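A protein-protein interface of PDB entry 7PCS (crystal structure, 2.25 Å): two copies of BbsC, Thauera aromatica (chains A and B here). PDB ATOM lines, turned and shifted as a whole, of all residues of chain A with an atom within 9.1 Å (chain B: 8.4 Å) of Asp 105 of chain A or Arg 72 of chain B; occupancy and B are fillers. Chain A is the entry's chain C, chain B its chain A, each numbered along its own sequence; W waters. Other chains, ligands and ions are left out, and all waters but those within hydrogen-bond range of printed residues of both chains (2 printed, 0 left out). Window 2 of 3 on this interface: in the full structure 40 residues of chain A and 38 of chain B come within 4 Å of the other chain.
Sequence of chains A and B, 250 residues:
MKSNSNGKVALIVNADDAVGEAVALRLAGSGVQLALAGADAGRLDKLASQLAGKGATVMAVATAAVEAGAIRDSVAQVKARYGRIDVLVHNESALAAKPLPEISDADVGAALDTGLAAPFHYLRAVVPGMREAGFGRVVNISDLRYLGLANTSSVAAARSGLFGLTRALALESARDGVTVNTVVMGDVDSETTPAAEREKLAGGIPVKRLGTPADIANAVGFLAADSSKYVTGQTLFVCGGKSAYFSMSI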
ATOM      1  N   LEU A 100     -29.966  -8.637 -33.515  1.00  0.00           N
ATOM      2  CA  LEU A 100     -29.379  -9.859 -32.967  1.00  0.00           C
ATOM      3  C   LEU A 100     -28.198  -9.610 -32.040  1.00  0.00           C
ATOM      4  O   LEU A 100     -28.161 -10.215 -30.960  1.00  0.00           O
ATOM      5  CB  LEU A 100     -28.973 -10.767 -34.136  1.00  0.00           C
ATOM      6  CG  LEU A 100     -28.657 -12.231 -33.837  1.00  0.00           C
ATOM      7  CD1 LEU A 100     -29.808 -12.884 -33.102  1.00  0.00           C
ATOM      8  CD2 LEU A 100     -28.360 -12.975 -35.147  1.00  0.00           C
ATOM      9  N   PRO A 101     -27.219  -8.768 -32.383  1.00  0.00           N
ATOM     10  CA  PRO A 101     -26.055  -8.610 -31.487  1.00  0.00           C
ATOM     11  C   PRO A 101     -26.419  -8.142 -30.088  1.00  0.00           C
ATOM     12  O   PRO A 101     -25.753  -8.520 -29.115  1.00  0.00           O
ATOM     13  CB  PRO A 101     -25.184  -7.572 -32.212  1.00  0.00           C
ATOM     14  CG  PRO A 101     -25.619  -7.646 -33.665  1.00  0.00           C
ATOM     15  CD  PRO A 101     -27.101  -7.945 -33.605  1.00  0.00           C
ATOM     16  N   GLU A 102     -27.443  -7.312 -29.955  1.00  0.00           N
ATOM     17  CA  GLU A 102     -27.829  -6.773 -28.663  1.00  0.00           C
ATOM     18  C   GLU A 102     -28.632  -7.754 -27.822  1.00  0.00           C
ATOM     19  O   GLU A 102     -28.998  -7.423 -26.685  1.00  0.00           O
ATOM     20  CB  GLU A 102     -28.653  -5.509 -28.901  1.00  0.00           C
ATOM     21  CG  GLU A 102     -27.856  -4.373 -29.540  1.00  0.00           C
ATOM     22  CD  GLU A 102     -28.712  -3.157 -29.820  1.00  0.00           C
ATOM     23  OE1 GLU A 102     -29.653  -2.920 -29.036  1.00  0.00           O
ATOM     24  OE2 GLU A 102     -28.440  -2.437 -30.808  1.00  0.00           O
ATOM     25  N   ILE A 103     -28.898  -8.948 -28.342  1.00  0.00           N
ATOM     26  CA  ILE A 103     -29.712  -9.939 -27.649  1.00  0.00           C
ATOM     27  C   ILE A 103     -28.807 -10.807 -26.785  1.00  0.00           C
ATOM     28  O   ILE A 103     -27.872 -11.444 -27.284  1.00  0.00           O
ATOM     29  CB  ILE A 103     -30.515 -10.789 -28.644  1.00  0.00           C
ATOM     30  CG1 ILE A 103     -31.340  -9.875 -29.551  1.00  0.00           C
ATOM     31  CG2 ILE A 103     -31.424 -11.748 -27.910  1.00  0.00           C
ATOM     32  CD1 ILE A 103     -32.222 -10.613 -30.554  1.00  0.00           C
ATOM     33  N   SER A 104     -29.085 -10.830 -25.490  1.00  0.00           N
ATOM     34  CA  SER A 104     -28.315 -11.598 -24.527  1.00  0.00           C
ATOM     35  C   SER A 104     -28.990 -12.932 -24.239  1.00  0.00           C
ATOM     36  O   SER A 104     -30.110 -13.203 -24.680  1.00  0.00           O
ATOM     37  CB  SER A 104     -28.151 -10.811 -23.230  1.00  0.00           C
ATOM     38  OG  SER A 104     -29.347 -10.883 -22.475  1.00  0.00           O
ATOM     39  N   ASP A 105     -28.287 -13.762 -23.463  1.00  0.00           N
ATOM     40  CA  ASP A 105     -28.832 -15.059 -23.069  1.00  0.00           C
ATOM     41  C   ASP A 105     -30.112 -14.900 -22.263  1.00  0.00           C
ATOM     42  O   ASP A 105     -31.025 -15.727 -22.376  1.00  0.00           O
ATOM     43  CB  ASP A 105     -27.792 -15.839 -22.258  1.00  0.00           C
ATOM     44  CG  ASP A 105     -26.664 -16.363 -23.115  1.00  0.00           C
ATOM     45  OD1 ASP A 105     -26.702 -16.132 -24.346  1.00  0.00           O
ATOM     46  OD2 ASP A 105     -25.738 -16.992 -22.558  1.00  0.00           O
ATOM     47  N   ALA A 106     -30.199 -13.850 -21.447  1.00  0.00           N
ATOM     48  CA  ALA A 106     -31.381 -13.639 -20.624  1.00  0.00           C
ATOM     49  C   ALA A 106     -32.490 -12.964 -21.409  1.00  0.00           C
ATOM     50  O   ALA A 106     -33.669 -13.186 -21.120  1.00  0.00           O
ATOM     51  CB  ALA A 106     -31.030 -12.808 -19.386  1.00  0.00           C
ATOM     52  N   ASP A 107     -32.138 -12.146 -22.405  1.00  0.00           N
ATOM     53  CA  ASP A 107     -33.158 -11.594 -23.292  1.00  0.00           C
ATOM     54  C   ASP A 107     -33.997 -12.698 -23.927  1.00  0.00           C
ATOM     55  O   ASP A 107     -35.218 -12.559 -24.071  1.00  0.00           O
ATOM     56  CB  ASP A 107     -32.508 -10.734 -24.379  1.00  0.00           C
ATOM     57  CG  ASP A 107     -31.959  -9.431 -23.843  1.00  0.00           C
ATOM     58  OD1 ASP A 107     -32.419  -8.999 -22.767  1.00  0.00           O
ATOM     59  OD2 ASP A 107     -31.074  -8.838 -24.499  1.00  0.00           O
ATOM     60  N   VAL A 108     -33.357 -13.795 -24.337  1.00  0.00           N
ATOM     61  CA  VAL A 108     -34.100 -14.897 -24.945  1.00  0.00           C
ATOM     62  C   VAL A 108     -35.060 -15.503 -23.931  1.00  0.00           C
ATOM     63  O   VAL A 108     -36.267 -15.610 -24.177  1.00  0.00           O
ATOM     64  CB  VAL A 108     -33.135 -15.955 -25.509  1.00  0.00           C
ATOM     65  CG1 VAL A 108     -33.908 -17.182 -25.984  1.00  0.00           C
ATOM     66  CG2 VAL A 108     -32.311 -15.372 -26.653  1.00  0.00           C
ATOM     67  N   GLY A 109     -34.539 -15.893 -22.768  1.00  0.00           N
ATOM     68  CA  GLY A 109     -35.377 -16.547 -21.776  1.00  0.00           C
ATOM     69  C   GLY A 109     -36.536 -15.682 -21.314  1.00  0.00           C
ATOM     70  O   GLY A 109     -37.650 -16.175 -21.119  1.00  0.00           O
ATOM     71  N   ALA A 110     -36.289 -14.386 -21.123  1.00  0.00           N
ATOM     72  CA  ALA A 110     -37.344 -13.496 -20.646  1.00  0.00           C
ATOM     73  C   ALA A 110     -38.453 -13.351 -21.685  1.00  0.00           C
ATOM     74  O   ALA A 110     -39.640 -13.463 -21.360  1.00  0.00           O
ATOM     75  CB  ALA A 110     -36.759 -12.129 -20.286  1.00  0.00           C
ATOM     76  N   ALA A 111     -38.082 -13.093 -22.941  1.00  0.00           N
ATOM     77  CA  ALA A 111     -39.081 -12.989 -24.003  1.00  0.00           C
ATOM     78  C   ALA A 111     -39.973 -14.223 -24.031  1.00  0.00           C
ATOM     79  O   ALA A 111     -41.203 -14.120 -24.109  1.00  0.00           O
ATOM     80  CB  ALA A 111     -38.391 -12.789 -25.352  1.00  0.00           C
ATOM     81  N   LEU A 112     -39.363 -15.408 -23.972  1.00  0.00           N
ATOM     82  CA  LEU A 112     -40.148 -16.636 -23.980  1.00  0.00           C
ATOM     83  C   LEU A 112     -41.030 -16.737 -22.740  1.00  0.00           C
ATOM     84  O   LEU A 112     -42.177 -17.191 -22.817  1.00  0.00           O
ATOM     85  CB  LEU A 112     -39.223 -17.851 -24.077  1.00  0.00           C
ATOM     86  CG  LEU A 112     -38.251 -17.906 -25.257  1.00  0.00           C
ATOM     87  CD1 LEU A 112     -37.615 -19.287 -25.363  1.00  0.00           C
ATOM     88  CD2 LEU A 112     -38.950 -17.528 -26.551  1.00  0.00           C
ATOM     89  N   ASP A 113     -40.508 -16.320 -21.584  1.00  0.00           N
ATOM     90  CA  ASP A 113     -41.242 -16.489 -20.334  1.00  0.00           C
ATOM     91  C   ASP A 113     -42.524 -15.665 -20.330  1.00  0.00           C
ATOM     92  O   ASP A 113     -43.610 -16.182 -20.040  1.00  0.00           O
ATOM     93  CB  ASP A 113     -40.351 -16.096 -19.154  1.00  0.00           C
ATOM     94  CG  ASP A 113     -39.345 -17.180 -18.786  1.00  0.00           C
ATOM     95  OD1 ASP A 113     -39.712 -18.378 -18.751  1.00  0.00           O
ATOM     96  OD2 ASP A 113     -38.173 -16.831 -18.534  1.00  0.00           O
ATOM     97  N   SER A 154     -35.969 -11.912 -31.066  1.00  0.00           N
ATOM     98  CA  SER A 154     -36.337 -12.356 -29.727  1.00  0.00           C
ATOM     99  C   SER A 154     -37.820 -12.145 -29.459  1.00  0.00           C
ATOM    100  O   SER A 154     -38.443 -12.947 -28.758  1.00  0.00           O
ATOM    101  CB  SER A 154     -35.500 -11.633 -28.670  1.00  0.00           C
ATOM    102  OG  SER A 154     -35.705 -10.233 -28.702  1.00  0.00           O
ATOM    103  N   THR B  63     -22.747 -33.477 -27.460  1.00  0.00           N
ATOM    104  CA  THR B  63     -23.312 -32.383 -26.685  1.00  0.00           C
ATOM    105  C   THR B  63     -24.821 -32.554 -26.599  1.00  0.00           C
ATOM    106  O   THR B  63     -25.500 -32.633 -27.628  1.00  0.00           O
ATOM    107  CB  THR B  63     -22.968 -31.031 -27.316  1.00  0.00           C
ATOM    108  OG1 THR B  63     -23.591 -29.986 -26.560  1.00  0.00           O
ATOM    109  CG2 THR B  63     -23.451 -30.969 -28.758  1.00  0.00           C
ATOM    110  N   ALA B  65     -26.660 -30.245 -25.015  1.00  0.00           N
ATOM    111  CA  ALA B  65     -26.828 -28.951 -24.377  1.00  0.00           C
ATOM    112  C   ALA B  65     -27.994 -28.178 -24.976  1.00  0.00           C
ATOM    113  O   ALA B  65     -28.302 -28.286 -26.168  1.00  0.00           O
ATOM    114  CB  ALA B  65     -25.548 -28.123 -24.505  1.00  0.00           C
ATOM    115  N   VAL B  66     -28.648 -27.395 -24.117  1.00  0.00           N
ATOM    116  CA  VAL B  66     -29.612 -26.388 -24.537  1.00  0.00           C
ATOM    117  C   VAL B  66     -29.310 -25.022 -23.941  1.00  0.00           C
ATOM    118  O   VAL B  66     -30.016 -24.057 -24.241  1.00  0.00           O
ATOM    119  CB  VAL B  66     -31.056 -26.811 -24.189  1.00  0.00           C
ATOM    120  CG1 VAL B  66     -31.516 -27.939 -25.110  1.00  0.00           C
ATOM    121  CG2 VAL B  66     -31.149 -27.231 -22.730  1.00  0.00           C
ATOM    122  N   GLU B  67     -28.272 -24.912 -23.109  1.00  0.00           N
ATOM    123  CA  GLU B  67     -27.875 -23.651 -22.504  1.00  0.00           C
ATOM    124  C   GLU B  67     -26.965 -22.920 -23.480  1.00  0.00           C
ATOM    125  O   GLU B  67     -26.124 -23.535 -24.144  1.00  0.00           O
ATOM    126  CB  GLU B  67     -27.157 -23.893 -21.174  1.00  0.00           C
ATOM    127  CG  GLU B  67     -26.901 -22.632 -20.357  1.00  0.00           C
ATOM    128  CD  GLU B  67     -25.598 -21.945 -20.710  1.00  0.00           C
ATOM    129  OE1 GLU B  67     -24.637 -22.647 -21.102  1.00  0.00           O
ATOM    130  OE2 GLU B  67     -25.538 -20.700 -20.592  1.00  0.00           O
ATOM    131  N   ALA B  68     -27.136 -21.601 -23.559  1.00  0.00           N
ATOM    132  CA  ALA B  68     -26.521 -20.838 -24.641  1.00  0.00           C
ATOM    133  C   ALA B  68     -25.004 -20.976 -24.625  1.00  0.00           C
ATOM    134  O   ALA B  68     -24.381 -21.204 -25.667  1.00  0.00           O
ATOM    135  CB  ALA B  68     -26.926 -19.365 -24.538  1.00  0.00           C
ATOM    136  N   GLY B  69     -24.387 -20.831 -23.451  1.00  0.00           N
ATOM    137  CA  GLY B  69     -22.933 -20.870 -23.382  1.00  0.00           C
ATOM    138  C   GLY B  69     -22.348 -22.158 -23.928  1.00  0.00           C
ATOM    139  O   GLY B  69     -21.375 -22.143 -24.688  1.00  0.00           O
ATOM    140  N   ALA B  70     -22.926 -23.295 -23.538  1.00  0.00           N
ATOM    141  CA  ALA B  70     -22.456 -24.578 -24.052  1.00  0.00           C
ATOM    142  C   ALA B  70     -22.596 -24.656 -25.570  1.00  0.00           C
ATOM    143  O   ALA B  70     -21.733 -25.222 -26.250  1.00  0.00           O
ATOM    144  CB  ALA B  70     -23.220 -25.718 -23.380  1.00  0.00           C
ATOM    145  N   ILE B  71     -23.679 -24.100 -26.118  1.00  0.00           N
ATOM    146  CA  ILE B  71     -23.885 -24.143 -27.564  1.00  0.00           C
ATOM    147  C   ILE B  71     -22.802 -23.336 -28.273  1.00  0.00           C
ATOM    148  O   ILE B  71     -22.225 -23.784 -29.274  1.00  0.00           O
ATOM    149  CB  ILE B  71     -25.296 -23.640 -27.920  1.00  0.00           C
ATOM    150  CG1 ILE B  71     -26.333 -24.715 -27.595  1.00  0.00           C
ATOM    151  CG2 ILE B  71     -25.376 -23.276 -29.390  1.00  0.00           C
ATOM    152  CD1 ILE B  71     -27.735 -24.175 -27.403  1.00  0.00           C
ATOM    153  N   ARG B  72     -22.515 -22.128 -27.773  1.00  0.00           N
ATOM    154  CA  ARG B  72     -21.459 -21.318 -28.374  1.00  0.00           C
ATOM    155  C   ARG B  72     -20.132 -22.056 -28.350  1.00  0.00           C
ATOM    156  O   ARG B  72     -19.324 -21.941 -29.283  1.00  0.00           O
ATOM    157  CB  ARG B  72     -21.358 -19.968 -27.652  1.00  0.00           C
ATOM    158  CG  ARG B  72     -22.630 -19.136 -27.740  1.00  0.00           C
ATOM    159  CD  ARG B  72     -22.368 -17.653 -27.516  1.00  0.00           C
ATOM    160  NE  ARG B  72     -22.317 -17.297 -26.102  1.00  0.00           N
ATOM    161  CZ  ARG B  72     -23.365 -17.327 -25.288  1.00  0.00           C
ATOM    162  NH1 ARG B  72     -24.562 -17.686 -25.720  1.00  0.00           N
ATOM    163  NH2 ARG B  72     -23.208 -16.982 -24.011  1.00  0.00           N
ATOM    164  N   ASP B  73     -19.893 -22.826 -27.292  1.00  0.00           N
ATOM    165  CA  ASP B  73     -18.669 -23.623 -27.243  1.00  0.00           C
ATOM    166  C   ASP B  73     -18.631 -24.637 -28.378  1.00  0.00           C
ATOM    167  O   ASP B  73     -17.651 -24.709 -29.130  1.00  0.00           O
ATOM    168  CB  ASP B  73     -18.515 -24.340 -25.897  1.00  0.00           C
ATOM    169  CG  ASP B  73     -17.783 -23.508 -24.860  1.00  0.00           C
ATOM    170  OD1 ASP B  73     -17.109 -22.517 -25.211  1.00  0.00           O
ATOM    171  OD2 ASP B  73     -17.873 -23.863 -23.670  1.00  0.00           O
ATOM    172  N   SER B  74     -19.681 -25.456 -28.491  1.00  0.00           N
ATOM    173  CA  SER B  74     -19.784 -26.392 -29.606  1.00  0.00           C
ATOM    174  C   SER B  74     -19.451 -25.712 -30.929  1.00  0.00           C
ATOM    175  O   SER B  74     -18.639 -26.214 -31.712  1.00  0.00           O
ATOM    176  CB  SER B  74     -21.186 -27.000 -29.652  1.00  0.00           C
ATOM    177  OG  SER B  74     -21.434 -27.815 -28.520  1.00  0.00           O
ATOM    178  N   VAL B  75     -20.053 -24.549 -31.183  1.00  0.00           N
ATOM    179  CA  VAL B  75     -19.800 -23.841 -32.434  1.00  0.00           C
ATOM    180  C   VAL B  75     -18.323 -23.498 -32.572  1.00  0.00           C
ATOM    181  O   VAL B  75     -17.740 -23.629 -33.656  1.00  0.00           O
ATOM    182  CB  VAL B  75     -20.682 -22.584 -32.522  1.00  0.00           C
ATOM    183  CG1 VAL B  75     -20.171 -21.646 -33.611  1.00  0.00           C
ATOM    184  CG2 VAL B  75     -22.131 -22.971 -32.767  1.00  0.00           C
ATOM    185  N   ALA B  76     -17.694 -23.048 -31.482  1.00  0.00           N
ATOM    186  CA  ALA B  76     -16.286 -22.673 -31.543  1.00  0.00           C
ATOM    187  C   ALA B  76     -15.414 -23.864 -31.920  1.00  0.00           C
ATOM    188  O   ALA B  76     -14.459 -23.721 -32.695  1.00  0.00           O
ATOM    189  CB  ALA B  76     -15.838 -22.081 -30.207  1.00  0.00           C
ATOM    190  N   GLN B  77     -15.717 -25.048 -31.379  1.00  0.00           N
ATOM    191  CA  GLN B  77     -14.975 -26.243 -31.773  1.00  0.00           C
ATOM    192  C   GLN B  77     -14.981 -26.395 -33.288  1.00  0.00           C
ATOM    193  O   GLN B  77     -13.934 -26.593 -33.913  1.00  0.00           O
ATOM    194  CB  GLN B  77     -15.564 -27.495 -31.120  1.00  0.00           C
ATOM    195  CG  GLN B  77     -15.637 -27.476 -29.612  1.00  0.00           C
ATOM    196  CD  GLN B  77     -15.830 -28.874 -29.040  1.00  0.00           C
ATOM    197  OE1 GLN B  77     -15.410 -29.871 -29.640  1.00  0.00           O
ATOM    198  NE2 GLN B  77     -16.477 -28.953 -27.875  1.00  0.00           N
ATOM    199  N   VAL B  78     -16.168 -26.316 -33.892  1.00  0.00           N
ATOM    200  CA  VAL B  78     -16.273 -26.431 -35.343  1.00  0.00           C
ATOM    201  C   VAL B  78     -15.426 -25.365 -36.015  1.00  0.00           C
ATOM    202  O   VAL B  78     -14.679 -25.644 -36.959  1.00  0.00           O
ATOM    203  CB  VAL B  78     -17.745 -26.345 -35.790  1.00  0.00           C
ATOM    204  CG1 VAL B  78     -17.869 -26.584 -37.275  1.00  0.00           C
ATOM    205  CG2 VAL B  78     -18.590 -27.362 -35.040  1.00  0.00           C
ATOM    206  N   LYS B  79     -15.554 -24.119 -35.562  1.00  0.00           N
ATOM    207  CA  LYS B  79     -14.806 -23.048 -36.207  1.00  0.00           C
ATOM    208  C   LYS B  79     -13.305 -23.210 -35.995  1.00  0.00           C
ATOM    209  O   LYS B  79     -12.510 -22.802 -36.851  1.00  0.00           O
ATOM    210  CB  LYS B  79     -15.260 -21.693 -35.671  1.00  0.00           C
ATOM    211  CG  LYS B  79     -16.615 -21.254 -36.163  1.00  0.00           C
ATOM    212  CD  LYS B  79     -16.836 -19.770 -35.863  1.00  0.00           C
ATOM    213  CE  LYS B  79     -18.186 -19.308 -36.402  1.00  0.00           C
ATOM    214  NZ  LYS B  79     -18.295 -17.825 -36.343  1.00  0.00           N
ATOM    215  N   ILE B  85     -18.214 -21.493 -40.869  1.00  0.00           N
ATOM    216  CA  ILE B  85     -19.438 -22.282 -40.983  1.00  0.00           C
ATOM    217  C   ILE B  85     -20.272 -21.670 -42.103  1.00  0.00           C
ATOM    218  O   ILE B  85     -20.881 -20.609 -41.922  1.00  0.00           O
ATOM    219  CB  ILE B  85     -20.231 -22.332 -39.669  1.00  0.00           C
ATOM    220  CG1 ILE B  85     -19.374 -22.976 -38.576  1.00  0.00           C
ATOM    221  CG2 ILE B  85     -21.554 -23.072 -39.893  1.00  0.00           C
ATOM    222  CD1 ILE B  85     -20.007 -22.948 -37.203  1.00  0.00           C
ATOM    223  N   ALA B 117     -35.471 -22.403 -27.737  1.00  0.00           N
ATOM    224  CA  ALA B 117     -34.332 -21.633 -27.249  1.00  0.00           C
ATOM    225  C   ALA B 117     -33.029 -22.177 -27.824  1.00  0.00           C
ATOM    226  O   ALA B 117     -32.172 -21.413 -28.287  1.00  0.00           O
ATOM    227  CB  ALA B 117     -34.295 -21.648 -25.720  1.00  0.00           C
ATOM    228  N   ALA B 118     -32.858 -23.499 -27.790  1.00  0.00           N
ATOM    229  CA  ALA B 118     -31.632 -24.099 -28.311  1.00  0.00           C
ATOM    230  C   ALA B 118     -31.373 -23.725 -29.763  1.00  0.00           C
ATOM    231  O   ALA B 118     -30.268 -23.240 -30.066  1.00  0.00           O
ATOM    232  CB  ALA B 118     -31.688 -25.618 -28.132  1.00  0.00           C
ATOM    233  N   PHE B 120     -32.464 -21.160 -31.428  1.00  0.00           N
ATOM    234  CA  PHE B 120     -32.159 -19.733 -31.369  1.00  0.00           C
ATOM    235  C   PHE B 120     -30.699 -19.507 -31.000  1.00  0.00           C
ATOM    236  O   PHE B 120     -29.983 -18.743 -31.659  1.00  0.00           O
ATOM    237  CB  PHE B 120     -33.077 -19.053 -30.350  1.00  0.00           C
ATOM    238  CG  PHE B 120     -33.185 -17.559 -30.509  1.00  0.00           C
ATOM    239  CD1 PHE B 120     -32.387 -16.871 -31.406  1.00  0.00           C
ATOM    240  CD2 PHE B 120     -34.088 -16.840 -29.745  1.00  0.00           C
ATOM    241  CE1 PHE B 120     -32.493 -15.490 -31.541  1.00  0.00           C
ATOM    242  CE2 PHE B 120     -34.200 -15.465 -29.878  1.00  0.00           C
ATOM    243  CZ  PHE B 120     -33.398 -14.790 -30.776  1.00  0.00           C
ATOM    244  N   HIS B 121     -30.237 -20.173 -29.942  1.00  0.00           N
ATOM    245  CA  HIS B 121     -28.864 -19.981 -29.493  1.00  0.00           C
ATOM    246  C   HIS B 121     -27.872 -20.382 -30.575  1.00  0.00           C
ATOM    247  O   HIS B 121     -26.852 -19.712 -30.771  1.00  0.00           O
ATOM    248  CB  HIS B 121     -28.618 -20.770 -28.210  1.00  0.00           C
ATOM    249  CG  HIS B 121     -29.407 -20.279 -27.034  1.00  0.00           C
ATOM    250  ND1 HIS B 121     -29.659 -18.941 -26.812  1.00  0.00           N
ATOM    251  CD2 HIS B 121     -29.994 -20.946 -26.012  1.00  0.00           C
ATOM    252  CE1 HIS B 121     -30.364 -18.806 -25.704  1.00  0.00           C
ATOM    253  NE2 HIS B 121     -30.575 -20.006 -25.194  1.00  0.00           N
ATOM    254  N   TYR B 122     -28.148 -21.476 -31.289  1.00  0.00           N
ATOM    255  CA  TYR B 122     -27.285 -21.844 -32.407  1.00  0.00           C
ATOM    256  C   TYR B 122     -27.287 -20.757 -33.475  1.00  0.00           C
ATOM    257  O   TYR B 122     -26.233 -20.401 -34.013  1.00  0.00           O
ATOM    258  CB  TYR B 122     -27.715 -23.188 -33.006  1.00  0.00           C
ATOM    259  CG  TYR B 122     -27.188 -24.401 -32.259  1.00  0.00           C
ATOM    260  CD1 TYR B 122     -25.882 -24.836 -32.443  1.00  0.00           C
ATOM    261  CD2 TYR B 122     -27.996 -25.118 -31.383  1.00  0.00           C
ATOM    262  CE1 TYR B 122     -25.386 -25.939 -31.763  1.00  0.00           C
ATOM    263  CE2 TYR B 122     -27.511 -26.226 -30.700  1.00  0.00           C
ATOM    264  CZ  TYR B 122     -26.203 -26.628 -30.894  1.00  0.00           C
ATOM    265  OH  TYR B 122     -25.711 -27.725 -30.228  1.00  0.00           O
ATOM    266  N   ARG B 124     -27.869 -17.565 -33.080  1.00  0.00           N
ATOM    267  CA  ARG B 124     -27.135 -16.416 -32.558  1.00  0.00           C
ATOM    268  C   ARG B 124     -25.632 -16.624 -32.661  1.00  0.00           C
ATOM    269  O   ARG B 124     -24.885 -15.665 -32.894  1.00  0.00           O
ATOM    270  CB  ARG B 124     -27.520 -16.167 -31.096  1.00  0.00           C
ATOM    271  CG  ARG B 124     -28.955 -15.678 -30.921  1.00  0.00           C
ATOM    272  CD  ARG B 124     -29.371 -15.624 -29.462  1.00  0.00           C
ATOM    273  NE  ARG B 124     -28.468 -14.810 -28.659  1.00  0.00           N
ATOM    274  CZ  ARG B 124     -28.083 -15.120 -27.430  1.00  0.00           C
ATOM    275  NH1 ARG B 124     -28.520 -16.213 -26.826  1.00  0.00           N
ATOM    276  NH2 ARG B 124     -27.235 -14.315 -26.794  1.00  0.00           N
ATOM    277  N   ALA B 125     -25.174 -17.866 -32.491  1.00  0.00           N
ATOM    278  CA  ALA B 125     -23.749 -18.167 -32.488  1.00  0.00           C
ATOM    279  C   ALA B 125     -23.154 -18.237 -33.884  1.00  0.00           C
ATOM    280  O   ALA B 125     -21.933 -18.114 -34.027  1.00  0.00           O
ATOM    281  CB  ALA B 125     -23.495 -19.490 -31.760  1.00  0.00           C
ATOM    282  N   VAL B 126     -23.979 -18.421 -34.910  1.00  0.00           N
ATOM    283  CA  VAL B 126     -23.504 -18.704 -36.255  1.00  0.00           C
ATOM    284  C   VAL B 126     -23.828 -17.571 -37.216  1.00  0.00           C
ATOM    285  O   VAL B 126     -23.000 -17.213 -38.055  1.00  0.00           O
ATOM    286  CB  VAL B 126     -24.089 -20.041 -36.766  1.00  0.00           C
ATOM    287  CG1 VAL B 126     -23.434 -20.445 -38.084  1.00  0.00           C
ATOM    288  CG2 VAL B 126     -23.940 -21.120 -35.709  1.00  0.00           C
HETATM  289  O   HOH W   1     -27.351 -12.788 -30.145  1.00  0.00           O
HETATM  290  O   HOH W   2     -31.511 -18.604 -22.669  1.00  0.00           O
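Printed residues of chain B within 4 Å of Leu 100 of chain A: Arg 124. Of the printed residues of chain B, Ile 103 of chain A touches Arg 124 (3.0 Å). Of chain B, only Arg 124 comes within 4 Å of Ser 104 of chain A. Asp 105 of chain A touches three residues of chain B. Ala 106 of chain A touches none of the printed residues of chain B. Of chain A, only Asp 105 comes within 4 Å of Arg 72 of chain B. No residue of chain A comes within 4 Å of Val 75 of chain B. Printed residues of chain A within 4 Å of Phe 120 of chain B: Val 108 (3.7 Å) and Ser 154 (3.8 Å). The nearest residue of chain A that does not touch Arg 72 of chain B is Ser 104 of chain A (6.7 Å). The nearest printed residue of chain B that does not touch Val 108 of chain A is Ala 117 of chain B (4.5 Å).
Along chain A the printed residues that touch a printed residue of chain B span positions 100 to 154. Printed residues of chain B that touch a printed residue of chain A: Ala 68, Arg 72, Phe 120, His 121 and Arg 124. Among the printed residues, 10 pairs touch across the chains. Among the printed residues, Asp or Glu carboxylates within 4 Å of a Lys or Arg side-chain nitrogen of the other chain: Asp 105 of chain A with Arg 72 of chain B (2.9 Å) and Asp 105 of chain A with Arg 124 of chain B (3.1 Å).
Water W1 lies within hydrogen-bond range of the guanidinium group of Arg 124 of chain B (2.7 Å), the backbone carbonyl oxygen of Leu 100 of chain A (2.8 Å) and the backbone carbonyl oxygen of Ile 103 of chain A (3.2 Å). Water W2 lies within hydrogen-bond range of the backbone carbonyl oxygen (O) of Asp 105 of chain A (2.9 Å) and a ring nitrogen (NE2) of His 121 of chain B (3.0 Å).
The guanidinium group (NH1) of Arg 124 of chain B lies within hydrogen-bond range of a ring nitrogen (ND1) of His 121 of chain B (3.0 Å). OG of Ser 104 of chain A sits close to N of Ala 106 of chain A (3.3 Å). The side-chain carboxylate (OD2) of Asp 107 of chain A is in hydrogen-bond range of the backbone NH (N) of Ser 104 of chain A (3.0 Å).
No position is printed for both chains. Of the 10 pairs that touch across the chains among the printed residues, none has its exchanged pair printed and touching as well.
The guanidinium group of Arg 72 of chain B is in salt-bridge range of the side-chain carboxylate of Asp 105 of chain A (2.9 Å). The guanidinium group (NH2) of Arg 124 of chain B is in hydrogen-bond range of the backbone carbonyl oxygen (O) of Ile 103 of chain A, 3.0 Å away. The side-chain carboxylate (OD1) of Asp 105 of chain A lies within salt-bridge range of the guanidinium group (NH1) of Arg 124 of chain B (3.1 Å).
Leu 100 of chain A touches Arg 124 of chain B (CD1 to CG, 3.6 Å). Ser 104 of chain A touches Arg 124 of chain B (C to NH2, 3.4 Å). Asp 105 of chain A touches Ala 68 of chain B (OD1 to CB, 3.2 Å). Phe 120 of chain B touches Val 108 of chain A. His 121 of chain B touches Val 108 of chain A. Arg 124 of chain B touches Val 108 of chain A. Ser 154 of chain A touches Phe 120 of chain B.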
